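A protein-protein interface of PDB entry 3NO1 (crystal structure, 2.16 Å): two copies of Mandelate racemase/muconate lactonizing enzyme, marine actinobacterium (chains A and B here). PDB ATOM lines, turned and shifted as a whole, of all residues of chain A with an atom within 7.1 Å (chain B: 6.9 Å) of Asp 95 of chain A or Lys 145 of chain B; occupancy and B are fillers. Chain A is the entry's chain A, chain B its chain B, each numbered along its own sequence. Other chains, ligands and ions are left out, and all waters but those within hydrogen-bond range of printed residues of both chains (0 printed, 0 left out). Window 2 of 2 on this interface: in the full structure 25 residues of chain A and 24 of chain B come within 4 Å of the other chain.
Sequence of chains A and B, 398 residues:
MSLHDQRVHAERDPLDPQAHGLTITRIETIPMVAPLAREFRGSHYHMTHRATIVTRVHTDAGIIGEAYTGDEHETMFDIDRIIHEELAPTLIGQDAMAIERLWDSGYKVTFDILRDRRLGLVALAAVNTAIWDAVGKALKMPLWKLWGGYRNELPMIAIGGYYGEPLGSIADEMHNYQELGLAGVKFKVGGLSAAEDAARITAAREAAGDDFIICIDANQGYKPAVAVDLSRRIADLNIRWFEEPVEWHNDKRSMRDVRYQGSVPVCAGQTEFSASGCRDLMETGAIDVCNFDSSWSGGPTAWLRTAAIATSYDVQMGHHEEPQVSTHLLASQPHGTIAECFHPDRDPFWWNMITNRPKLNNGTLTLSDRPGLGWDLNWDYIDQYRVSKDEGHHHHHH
N of Leu 22 of chain A is in hydrogen-bond range of OD1 of Asp 95 of chain A.
OD1 of Asp 95 of chain A lies within hydrogen-bond range of N of Met 97 of chain A (2.9 Å).
The backbone carbonyl oxygen of Trp 144 of chain B is in hydrogen-bond range of the backbone NH of Gly 149 of chain B (2.9 Å).
The backbone NH of Gly 149 of chain B is in hydrogen-bond range of the backbone carbonyl oxygen of Ser 332 of chain B.
O of Ser 332 of chain B lies within hydrogen-bond range of N of Tyr 150 of chain B.
No position is printed for both chains.
Of the 10 pairs that touch across the chains among the printed residues, none has its exchanged pair printed and touching as well.
Hydrophobic or aromatic side chains of chain B that line the printed part of chain A: Met 141 and Tyr 150.
Among the printed residues, 10 pairs touch across the chains.
Among the printed residues, Asp or Glu carboxylates within 4 Å of a Lys or Arg side-chain nitrogen of the other chain: Asp 95 of chain A with Lys 145 of chain B (3.9 Å).
The side-chain amino group (NZ) of Lys 145 of chain B is in salt-bridge range of the side-chain carboxylate (OD2) of Asp 95 of chain A, at 3.9 Å.
The backbone NH of Glu 100 of chain A is in hydrogen-bond range of the backbone carbonyl oxygen of Gly 148 of chain B, at 2.9 Å.
O of Gly 149 of chain B is in hydrogen-bond range of NH1 of Arg 101 of chain A, 2.9 Å away.
NH1 of Arg 101 of chain A is in hydrogen-bond range of O of Tyr 150 of chain B, at 3.1 Å.
Met 141 of chain B touches Met 97 of chain A.
Lys 145 of chain B touches Met 97 of chain A.
O of Gly 148 of chain B touches C of Ala 98 of chain A (3.7 Å).
Ala 98 of chain A touches Gly 149 of chain B.
N of Ile 99 of chain A touches O of Gly 148 of chain B (3.5 Å).
Ser 332 of chain B touches Glu 100 of chain A.
Of the printed residues of chain B, Ala 98 of chain A touches Gly 148 (3.7 Å) and Gly 149 (3.4 Å).
Of the printed residues of chain B, Ile 99 of chain A touches Gly 148 (3.5 Å).
Printed residues of chain B within 4 Å of Glu 100 of chain A: Gly 148 and Ser 332.
Lys 145 of chain B touches just these residues of chain A: Asp 95 and Met 97.
Of the printed residues of chain A, Gly 148 of chain B touches Ala 98, Ile 99 and Glu 100.
The nearest residue of chain B that does not touch Asp 95 of chain A is Trp 144 of chain B (6.5 Å).
The nearest residue of chain A that does not touch Lys 145 of chain B is Ala 98 of chain A (5.1 Å).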
ATOM      1  N   LEU A  22     -20.645  20.470 -26.786  1.00  0.00           N
ATOM      2  CA  LEU A  22     -19.531  21.348 -27.239  1.00  0.00           C
ATOM      3  C   LEU A  22     -19.744  22.779 -26.766  1.00  0.00           C
ATOM      4  O   LEU A  22     -20.769  23.405 -27.046  1.00  0.00           O
ATOM      5  CB  LEU A  22     -19.402  21.290 -28.763  1.00  0.00           C
ATOM      6  CG  LEU A  22     -20.477  21.870 -29.674  1.00  0.00           C
ATOM      7  CD1 LEU A  22     -20.385  23.383 -29.680  1.00  0.00           C
ATOM      8  CD2 LEU A  22     -20.261  21.353 -31.080  1.00  0.00           C
ATOM      9  N   THR A  23     -18.755  23.295 -26.049  1.00  0.00           N
ATOM     10  CA  THR A  23     -18.828  24.632 -25.484  1.00  0.00           C
ATOM     11  C   THR A  23     -18.556  25.752 -26.478  1.00  0.00           C
ATOM     12  O   THR A  23     -17.660  25.654 -27.311  1.00  0.00           O
ATOM     13  CB  THR A  23     -17.848  24.758 -24.299  1.00  0.00           C
ATOM     14  OG1 THR A  23     -18.091  23.693 -23.373  1.00  0.00           O
ATOM     15  CG2 THR A  23     -18.025  26.086 -23.592  1.00  0.00           C
ATOM     16  N   ILE A  24     -19.350  26.815 -26.371  1.00  0.00           N
ATOM     17  CA  ILE A  24     -19.221  27.989 -27.227  1.00  0.00           C
ATOM     18  C   ILE A  24     -18.159  28.907 -26.626  1.00  0.00           C
ATOM     19  O   ILE A  24     -18.240  29.276 -25.454  1.00  0.00           O
ATOM     20  CB  ILE A  24     -20.559  28.747 -27.322  1.00  0.00           C
ATOM     21  CG1 ILE A  24     -21.594  27.871 -28.043  1.00  0.00           C
ATOM     22  CG2 ILE A  24     -20.361  30.071 -28.039  1.00  0.00           C
ATOM     23  CD1 ILE A  24     -22.966  28.494 -28.132  1.00  0.00           C
ATOM     24  N   THR A  90     -25.632  34.936 -23.332  1.00  0.00           N
ATOM     25  CA  THR A  90     -26.414  33.736 -23.049  1.00  0.00           C
ATOM     26  C   THR A  90     -25.820  32.524 -23.749  1.00  0.00           C
ATOM     27  O   THR A  90     -26.287  31.398 -23.560  1.00  0.00           O
ATOM     28  CB  THR A  90     -27.883  33.888 -23.517  1.00  0.00           C
ATOM     29  OG1 THR A  90     -27.929  33.928 -24.950  1.00  0.00           O
ATOM     30  CG2 THR A  90     -28.486  35.172 -22.973  1.00  0.00           C
ATOM     31  N   LEU A  91     -24.788  32.755 -24.555  1.00  0.00           N
ATOM     32  CA  LEU A  91     -24.153  31.674 -25.307  1.00  0.00           C
ATOM     33  C   LEU A  91     -22.719  31.329 -24.888  1.00  0.00           C
ATOM     34  O   LEU A  91     -22.343  30.156 -24.886  1.00  0.00           O
ATOM     35  CB  LEU A  91     -24.166  32.016 -26.799  1.00  0.00           C
ATOM     36  CG  LEU A  91     -25.531  32.299 -27.431  1.00  0.00           C
ATOM     37  CD1 LEU A  91     -25.354  32.834 -28.843  1.00  0.00           C
ATOM     38  CD2 LEU A  91     -26.347  31.023 -27.438  1.00  0.00           C
ATOM     39  N   ILE A  92     -21.916  32.336 -24.547  1.00  0.00           N
ATOM     40  CA  ILE A  92     -20.522  32.089 -24.165  1.00  0.00           C
ATOM     41  C   ILE A  92     -20.410  31.115 -22.992  1.00  0.00           C
ATOM     42  O   ILE A  92     -21.025  31.315 -21.943  1.00  0.00           O
ATOM     43  CB  ILE A  92     -19.778  33.407 -23.800  1.00  0.00           C
ATOM     44  CG1 ILE A  92     -19.807  34.376 -24.988  1.00  0.00           C
ATOM     45  CG2 ILE A  92     -18.317  33.103 -23.415  1.00  0.00           C
ATOM     46  CD1 ILE A  92     -19.190  33.823 -26.261  1.00  0.00           C
ATOM     47  N   GLY A  93     -19.634  30.055 -23.188  1.00  0.00           N
ATOM     48  CA  GLY A  93     -19.453  29.059 -22.150  1.00  0.00           C
ATOM     49  C   GLY A  93     -20.574  28.039 -22.080  1.00  0.00           C
ATOM     50  O   GLY A  93     -20.506  27.104 -21.283  1.00  0.00           O
ATOM     51  N   GLN A  94     -21.602  28.208 -22.912  1.00  0.00           N
ATOM     52  CA  GLN A  94     -22.741  27.288 -22.923  1.00  0.00           C
ATOM     53  C   GLN A  94     -22.547  26.140 -23.910  1.00  0.00           C
ATOM     54  O   GLN A  94     -21.707  26.216 -24.811  1.00  0.00           O
ATOM     55  CB  GLN A  94     -24.033  28.034 -23.284  1.00  0.00           C
ATOM     56  CG  GLN A  94     -24.478  29.088 -22.281  1.00  0.00           C
ATOM     57  CD  GLN A  94     -24.811  28.501 -20.922  1.00  0.00           C
ATOM     58  OE1 GLN A  94     -24.045  28.634 -19.977  1.00  0.00           O
ATOM     59  NE2 GLN A  94     -25.959  27.839 -20.823  1.00  0.00           N
ATOM     60  N   ASP A  95     -23.343  25.087 -23.737  1.00  0.00           N
ATOM     61  CA  ASP A  95     -23.293  23.908 -24.596  1.00  0.00           C
ATOM     62  C   ASP A  95     -24.169  24.124 -25.829  1.00  0.00           C
ATOM     63  O   ASP A  95     -25.397  24.167 -25.729  1.00  0.00           O
ATOM     64  CB  ASP A  95     -23.787  22.677 -23.822  1.00  0.00           C
ATOM     65  CG  ASP A  95     -23.740  21.397 -24.654  1.00  0.00           C
ATOM     66  OD1 ASP A  95     -23.223  21.438 -25.787  1.00  0.00           O
ATOM     67  OD2 ASP A  95     -24.212  20.350 -24.169  1.00  0.00           O
ATOM     68  N   ALA A  96     -23.531  24.254 -26.989  1.00  0.00           N
ATOM     69  CA  ALA A  96     -24.252  24.471 -28.235  1.00  0.00           C
ATOM     70  C   ALA A  96     -25.208  23.329 -28.596  1.00  0.00           C
ATOM     71  O   ALA A  96     -26.096  23.511 -29.420  1.00  0.00           O
ATOM     72  CB  ALA A  96     -23.269  24.692 -29.368  1.00  0.00           C
ATOM     73  N   MET A  97     -25.025  22.162 -27.983  1.00  0.00           N
ATOM     74  CA  MET A  97     -25.879  21.004 -28.263  1.00  0.00           C
ATOM     75  C   MET A  97     -27.264  21.107 -27.618  1.00  0.00           C
ATOM     76  O   MET A  97     -28.164  20.337 -27.957  1.00  0.00           O
ATOM     77  CB  MET A  97     -25.218  19.708 -27.778  1.00  0.00           C
ATOM     78  CG  MET A  97     -23.890  19.371 -28.430  1.00  0.00           C
ATOM     79  SD  MET A  97     -24.034  19.142 -30.347  1.00  0.00           S
ATOM     80  CE  MET A  97     -24.155  17.238 -30.437  1.00  0.00           C
ATOM     81  N   ALA A  98     -27.423  22.036 -26.678  1.00  0.00           N
ATOM     82  CA  ALA A  98     -28.698  22.226 -25.988  1.00  0.00           C
ATOM     83  C   ALA A  98     -29.467  23.342 -26.679  1.00  0.00           C
ATOM     84  O   ALA A  98     -29.781  24.359 -26.070  1.00  0.00           O
ATOM     85  CB  ALA A  98     -28.449  22.587 -24.519  1.00  0.00           C
ATOM     86  N   ILE A  99     -29.776  23.141 -27.954  1.00  0.00           N
ATOM     87  CA  ILE A  99     -30.468  24.151 -28.738  1.00  0.00           C
ATOM     88  C   ILE A  99     -31.753  24.716 -28.151  1.00  0.00           C
ATOM     89  O   ILE A  99     -31.955  25.926 -28.193  1.00  0.00           O
ATOM     90  CB  ILE A  99     -30.743  23.642 -30.159  1.00  0.00           C
ATOM     91  CG1 ILE A  99     -29.404  23.347 -30.842  1.00  0.00           C
ATOM     92  CG2 ILE A  99     -31.542  24.683 -30.947  1.00  0.00           C
ATOM     93  CD1 ILE A  99     -29.486  23.111 -32.328  1.00  0.00           C
ATOM     94  N   GLU A 100     -32.619  23.867 -27.607  1.00  0.00           N
ATOM     95  CA  GLU A 100     -33.868  24.369 -27.032  1.00  0.00           C
ATOM     96  C   GLU A 100     -33.583  25.271 -25.828  1.00  0.00           C
ATOM     97  O   GLU A 100     -34.260  26.282 -25.613  1.00  0.00           O
ATOM     98  CB  GLU A 100     -34.774  23.211 -26.605  1.00  0.00           C
ATOM     99  CG  GLU A 100     -35.401  22.424 -27.760  1.00  0.00           C
ATOM    100  CD  GLU A 100     -36.365  23.250 -28.607  1.00  0.00           C
ATOM    101  OE1 GLU A 100     -36.763  24.359 -28.189  1.00  0.00           O
ATOM    102  OE2 GLU A 100     -36.736  22.776 -29.698  1.00  0.00           O
ATOM    103  N   ARG A 101     -32.570  24.913 -25.050  1.00  0.00           N
ATOM    104  CA  ARG A 101     -32.220  25.704 -23.876  1.00  0.00           C
ATOM    105  C   ARG A 101     -31.685  27.073 -24.274  1.00  0.00           C
ATOM    106  O   ARG A 101     -32.105  28.086 -23.720  1.00  0.00           O
ATOM    107  CB  ARG A 101     -31.196  24.957 -23.008  1.00  0.00           C
ATOM    108  CG  ARG A 101     -30.981  25.603 -21.645  1.00  0.00           C
ATOM    109  CD  ARG A 101     -30.494  24.587 -20.623  1.00  0.00           C
ATOM    110  NE  ARG A 101     -29.126  24.154 -20.878  1.00  0.00           N
ATOM    111  CZ  ARG A 101     -28.764  22.895 -21.109  1.00  0.00           C
ATOM    112  NH1 ARG A 101     -29.672  21.926 -21.120  1.00  0.00           N
ATOM    113  NH2 ARG A 101     -27.487  22.604 -21.327  1.00  0.00           N
ATOM    114  N   LEU A 102     -30.778  27.115 -25.249  1.00  0.00           N
ATOM    115  CA  LEU A 102     -30.207  28.389 -25.691  1.00  0.00           C
ATOM    116  C   LEU A 102     -31.234  29.291 -26.371  1.00  0.00           C
ATOM    117  O   LEU A 102     -31.318  30.488 -26.087  1.00  0.00           O
ATOM    118  CB  LEU A 102     -29.045  28.156 -26.658  1.00  0.00           C
ATOM    119  CG  LEU A 102     -27.871  27.322 -26.149  1.00  0.00           C
ATOM    120  CD1 LEU A 102     -26.781  27.314 -27.203  1.00  0.00           C
ATOM    121  CD2 LEU A 102     -27.349  27.900 -24.851  1.00  0.00           C
ATOM    122  N   ILE A 131     -25.395  28.204 -34.898  1.00  0.00           N
ATOM    123  CA  ILE A 131     -25.327  27.123 -33.926  1.00  0.00           C
ATOM    124  C   ILE A 131     -25.690  25.788 -34.580  1.00  0.00           C
ATOM    125  O   ILE A 131     -25.008  24.778 -34.375  1.00  0.00           O
ATOM    126  CB  ILE A 131     -26.268  27.402 -32.739  1.00  0.00           C
ATOM    127  CG1 ILE A 131     -25.752  28.609 -31.960  1.00  0.00           C
ATOM    128  CG2 ILE A 131     -26.368  26.177 -31.836  1.00  0.00           C
ATOM    129  CD1 ILE A 131     -26.700  29.115 -30.892  1.00  0.00           C
ATOM    130  N   MET B 141     -25.543  10.344 -29.368  1.00  0.00           N
ATOM    131  CA  MET B 141     -26.340  11.355 -28.686  1.00  0.00           C
ATOM    132  C   MET B 141     -27.520  10.793 -27.904  1.00  0.00           C
ATOM    133  O   MET B 141     -28.276   9.971 -28.415  1.00  0.00           O
ATOM    134  CB  MET B 141     -26.896  12.353 -29.707  1.00  0.00           C
ATOM    135  CG  MET B 141     -25.887  13.324 -30.282  1.00  0.00           C
ATOM    136  SD  MET B 141     -25.469  14.721 -29.024  1.00  0.00           S
ATOM    137  CE  MET B 141     -26.970  15.904 -29.390  1.00  0.00           C
ATOM    138  N   PRO B 142     -27.685  11.225 -26.644  1.00  0.00           N
ATOM    139  CA  PRO B 142     -28.820  10.734 -25.860  1.00  0.00           C
ATOM    140  C   PRO B 142     -30.053  11.438 -26.441  1.00  0.00           C
ATOM    141  O   PRO B 142     -29.988  12.620 -26.787  1.00  0.00           O
ATOM    142  CB  PRO B 142     -28.489  11.201 -24.444  1.00  0.00           C
ATOM    143  CG  PRO B 142     -27.705  12.452 -24.676  1.00  0.00           C
ATOM    144  CD  PRO B 142     -26.801  12.067 -25.823  1.00  0.00           C
ATOM    145  N   LEU B 143     -31.166  10.723 -26.563  1.00  0.00           N
ATOM    146  CA  LEU B 143     -32.368  11.314 -27.143  1.00  0.00           C
ATOM    147  C   LEU B 143     -32.877  12.606 -26.487  1.00  0.00           C
ATOM    148  O   LEU B 143     -33.305  13.520 -27.194  1.00  0.00           O
ATOM    149  CB  LEU B 143     -33.495  10.276 -27.197  1.00  0.00           C
ATOM    150  CG  LEU B 143     -33.736   9.455 -28.474  1.00  0.00           C
ATOM    151  CD1 LEU B 143     -32.832   9.905 -29.612  1.00  0.00           C
ATOM    152  CD2 LEU B 143     -33.527   7.988 -28.175  1.00  0.00           C
ATOM    153  N   TRP B 144     -32.829  12.707 -25.160  1.00  0.00           N
ATOM    154  CA  TRP B 144     -33.314  13.929 -24.522  1.00  0.00           C
ATOM    155  C   TRP B 144     -32.546  15.141 -25.044  1.00  0.00           C
ATOM    156  O   TRP B 144     -33.074  16.257 -25.085  1.00  0.00           O
ATOM    157  CB  TRP B 144     -33.193  13.864 -22.994  1.00  0.00           C
ATOM    158  CG  TRP B 144     -31.784  13.740 -22.467  1.00  0.00           C
ATOM    159  CD1 TRP B 144     -31.136  12.588 -22.116  1.00  0.00           C
ATOM    160  CD2 TRP B 144     -30.858  14.810 -22.222  1.00  0.00           C
ATOM    161  NE1 TRP B 144     -29.871  12.874 -21.663  1.00  0.00           N
ATOM    162  CE2 TRP B 144     -29.674  14.229 -21.718  1.00  0.00           C
ATOM    163  CE3 TRP B 144     -30.916  16.202 -22.380  1.00  0.00           C
ATOM    164  CZ2 TRP B 144     -28.552  14.995 -21.368  1.00  0.00           C
ATOM    165  CZ3 TRP B 144     -29.802  16.963 -22.032  1.00  0.00           C
ATOM    166  CH2 TRP B 144     -28.636  16.356 -21.531  1.00  0.00           C
ATOM    167  N   LYS B 145     -31.299  14.923 -25.450  1.00  0.00           N
ATOM    168  CA  LYS B 145     -30.503  16.023 -25.972  1.00  0.00           C
ATOM    169  C   LYS B 145     -30.725  16.180 -27.476  1.00  0.00           C
ATOM    170  O   LYS B 145     -30.874  17.299 -27.971  1.00  0.00           O
ATOM    171  CB  LYS B 145     -29.013  15.815 -25.676  1.00  0.00           C
ATOM    172  CG  LYS B 145     -28.150  17.026 -26.038  1.00  0.00           C
ATOM    173  CD  LYS B 145     -26.675  16.824 -25.668  1.00  0.00           C
ATOM    174  CE  LYS B 145     -26.456  16.874 -24.163  1.00  0.00           C
ATOM    175  NZ  LYS B 145     -25.052  16.532 -23.779  1.00  0.00           N
ATOM    176  N   LEU B 146     -30.766  15.065 -28.197  1.00  0.00           N
ATOM    177  CA  LEU B 146     -30.972  15.120 -29.642  1.00  0.00           C
ATOM    178  C   LEU B 146     -32.327  15.729 -30.013  1.00  0.00           C
ATOM    179  O   LEU B 146     -32.475  16.317 -31.083  1.00  0.00           O
ATOM    180  CB  LEU B 146     -30.872  13.727 -30.254  1.00  0.00           C
ATOM    181  CG  LEU B 146     -30.991  13.658 -31.783  1.00  0.00           C
ATOM    182  CD1 LEU B 146     -29.856  14.445 -32.452  1.00  0.00           C
ATOM    183  CD2 LEU B 146     -30.950  12.211 -32.206  1.00  0.00           C
ATOM    184  N   TRP B 147     -33.308  15.597 -29.122  1.00  0.00           N
ATOM    185  CA  TRP B 147     -34.644  16.129 -29.383  1.00  0.00           C
ATOM    186  C   TRP B 147     -34.822  17.578 -28.932  1.00  0.00           C
ATOM    187  O   TRP B 147     -35.907  18.149 -29.074  1.00  0.00           O
ATOM    188  CB  TRP B 147     -35.719  15.249 -28.719  1.00  0.00           C
ATOM    189  CG  TRP B 147     -35.923  13.908 -29.377  1.00  0.00           C
ATOM    190  CD1 TRP B 147     -35.739  13.601 -30.699  1.00  0.00           C
ATOM    191  CD2 TRP B 147     -36.449  12.720 -28.763  1.00  0.00           C
ATOM    192  NE1 TRP B 147     -36.121  12.302 -30.944  1.00  0.00           N
ATOM    193  CE2 TRP B 147     -36.560  11.739 -29.775  1.00  0.00           C
ATOM    194  CE3 TRP B 147     -36.839  12.392 -27.455  1.00  0.00           C
ATOM    195  CZ2 TRP B 147     -37.046  10.448 -29.519  1.00  0.00           C
ATOM    196  CZ3 TRP B 147     -37.323  11.107 -27.201  1.00  0.00           C
ATOM    197  CH2 TRP B 147     -37.421  10.152 -28.232  1.00  0.00           C
ATOM    198  N   GLY B 148     -33.768  18.178 -28.389  1.00  0.00           N
ATOM    199  CA  GLY B 148     -33.875  19.561 -27.962  1.00  0.00           C
ATOM    200  C   GLY B 148     -32.931  19.936 -26.837  1.00  0.00           C
ATOM    201  O   GLY B 148     -32.392  21.040 -26.814  1.00  0.00           O
ATOM    202  N   GLY B 149     -32.748  19.016 -25.897  1.00  0.00           N
ATOM    203  CA  GLY B 149     -31.845  19.250 -24.786  1.00  0.00           C
ATOM    204  C   GLY B 149     -32.185  20.392 -23.851  1.00  0.00           C
ATOM    205  O   GLY B 149     -31.277  21.034 -23.320  1.00  0.00           O
ATOM    206  N   TYR B 150     -33.470  20.663 -23.634  1.00  0.00           N
ATOM    207  CA  TYR B 150     -33.824  21.743 -22.729  1.00  0.00           C
ATOM    208  C   TYR B 150     -33.258  21.462 -21.334  1.00  0.00           C
ATOM    209  O   TYR B 150     -32.710  22.353 -20.698  1.00  0.00           O
ATOM    210  CB  TYR B 150     -35.335  21.919 -22.626  1.00  0.00           C
ATOM    211  CG  TYR B 150     -35.700  23.059 -21.711  1.00  0.00           C
ATOM    212  CD1 TYR B 150     -35.454  24.382 -22.084  1.00  0.00           C
ATOM    213  CD2 TYR B 150     -36.258  22.819 -20.456  1.00  0.00           C
ATOM    214  CE1 TYR B 150     -35.748  25.441 -21.224  1.00  0.00           C
ATOM    215  CE2 TYR B 150     -36.555  23.866 -19.591  1.00  0.00           C
ATOM    216  CZ  TYR B 150     -36.301  25.174 -19.983  1.00  0.00           C
ATOM    217  OH  TYR B 150     -36.596  26.215 -19.136  1.00  0.00           O
ATOM    218  N   ARG B 151     -33.417  20.226 -20.863  1.00  0.00           N
ATOM    219  CA  ARG B 151     -32.904  19.805 -19.559  1.00  0.00           C
ATOM    220  C   ARG B 151     -32.771  18.282 -19.552  1.00  0.00           C
ATOM    221  O   ARG B 151     -33.218  17.614 -20.488  1.00  0.00           O
ATOM    222  CB  ARG B 151     -33.839  20.254 -18.427  1.00  0.00           C
ATOM    223  CG  ARG B 151     -35.274  19.777 -18.573  1.00  0.00           C
ATOM    224  CD  ARG B 151     -36.107  20.088 -17.334  1.00  0.00           C
ATOM    225  NE  ARG B 151     -37.536  19.910 -17.587  1.00  0.00           N
ATOM    226  CZ  ARG B 151     -38.476  19.866 -16.646  1.00  0.00           C
ATOM    227  NH1 ARG B 151     -38.149  19.980 -15.364  1.00  0.00           N
ATOM    228  NH2 ARG B 151     -39.750  19.718 -16.990  1.00  0.00           N
ATOM    229  N   HIS B 328     -37.328  11.148 -21.948  1.00  0.00           N
ATOM    230  CA  HIS B 328     -36.503  11.820 -22.951  1.00  0.00           C
ATOM    231  C   HIS B 328     -37.319  12.873 -23.698  1.00  0.00           C
ATOM    232  O   HIS B 328     -36.859  13.994 -23.907  1.00  0.00           O
ATOM    233  CB  HIS B 328     -35.949  10.807 -23.959  1.00  0.00           C
ATOM    234  CG  HIS B 328     -34.842   9.954 -23.422  1.00  0.00           C
ATOM    235  ND1 HIS B 328     -33.546  10.406 -23.298  1.00  0.00           N
ATOM    236  CD2 HIS B 328     -34.839   8.676 -22.970  1.00  0.00           C
ATOM    237  CE1 HIS B 328     -32.794   9.444 -22.795  1.00  0.00           C
ATOM    238  NE2 HIS B 328     -33.554   8.385 -22.588  1.00  0.00           N
ATOM    239  N   ALA B 331     -38.163  15.869 -21.229  1.00  0.00           N
ATOM    240  CA  ALA B 331     -36.978  16.624 -20.811  1.00  0.00           C
ATOM    241  C   ALA B 331     -36.398  17.487 -21.928  1.00  0.00           C
ATOM    242  O   ALA B 331     -35.887  18.574 -21.680  1.00  0.00           O
ATOM    243  CB  ALA B 331     -35.899  15.663 -20.280  1.00  0.00           C
ATOM    244  N   SER B 332     -36.503  17.009 -23.162  1.00  0.00           N
ATOM    245  CA  SER B 332     -35.960  17.726 -24.316  1.00  0.00           C
ATOM    246  C   SER B 332     -36.628  19.070 -24.610  1.00  0.00           C
ATOM    247  O   SER B 332     -36.012  19.954 -25.217  1.00  0.00           O
ATOM    248  CB  SER B 332     -36.058  16.837 -25.567  1.00  0.00           C
ATOM    249  OG  SER B 332     -37.377  16.825 -26.093  1.00  0.00           O
ATOM    250  N   ASP B 369     -26.053  10.405 -20.127  1.00  0.00           N
ATOM    251  CA  ASP B 369     -25.580  10.847 -21.432  1.00  0.00           C
ATOM    252  C   ASP B 369     -25.521   9.663 -22.396  1.00  0.00           C
ATOM    253  O   ASP B 369     -25.084   9.805 -23.535  1.00  0.00           O
ATOM    254  CB  ASP B 369     -24.193  11.492 -21.311  1.00  0.00           C
ATOM    255  CG  ASP B 369     -24.248  12.938 -20.825  1.00  0.00           C
ATOM    256  OD1 ASP B 369     -23.169  13.544 -20.653  1.00  0.00           O
ATOM    257  OD2 ASP B 369     -25.356  13.477 -20.619  1.00  0.00           O
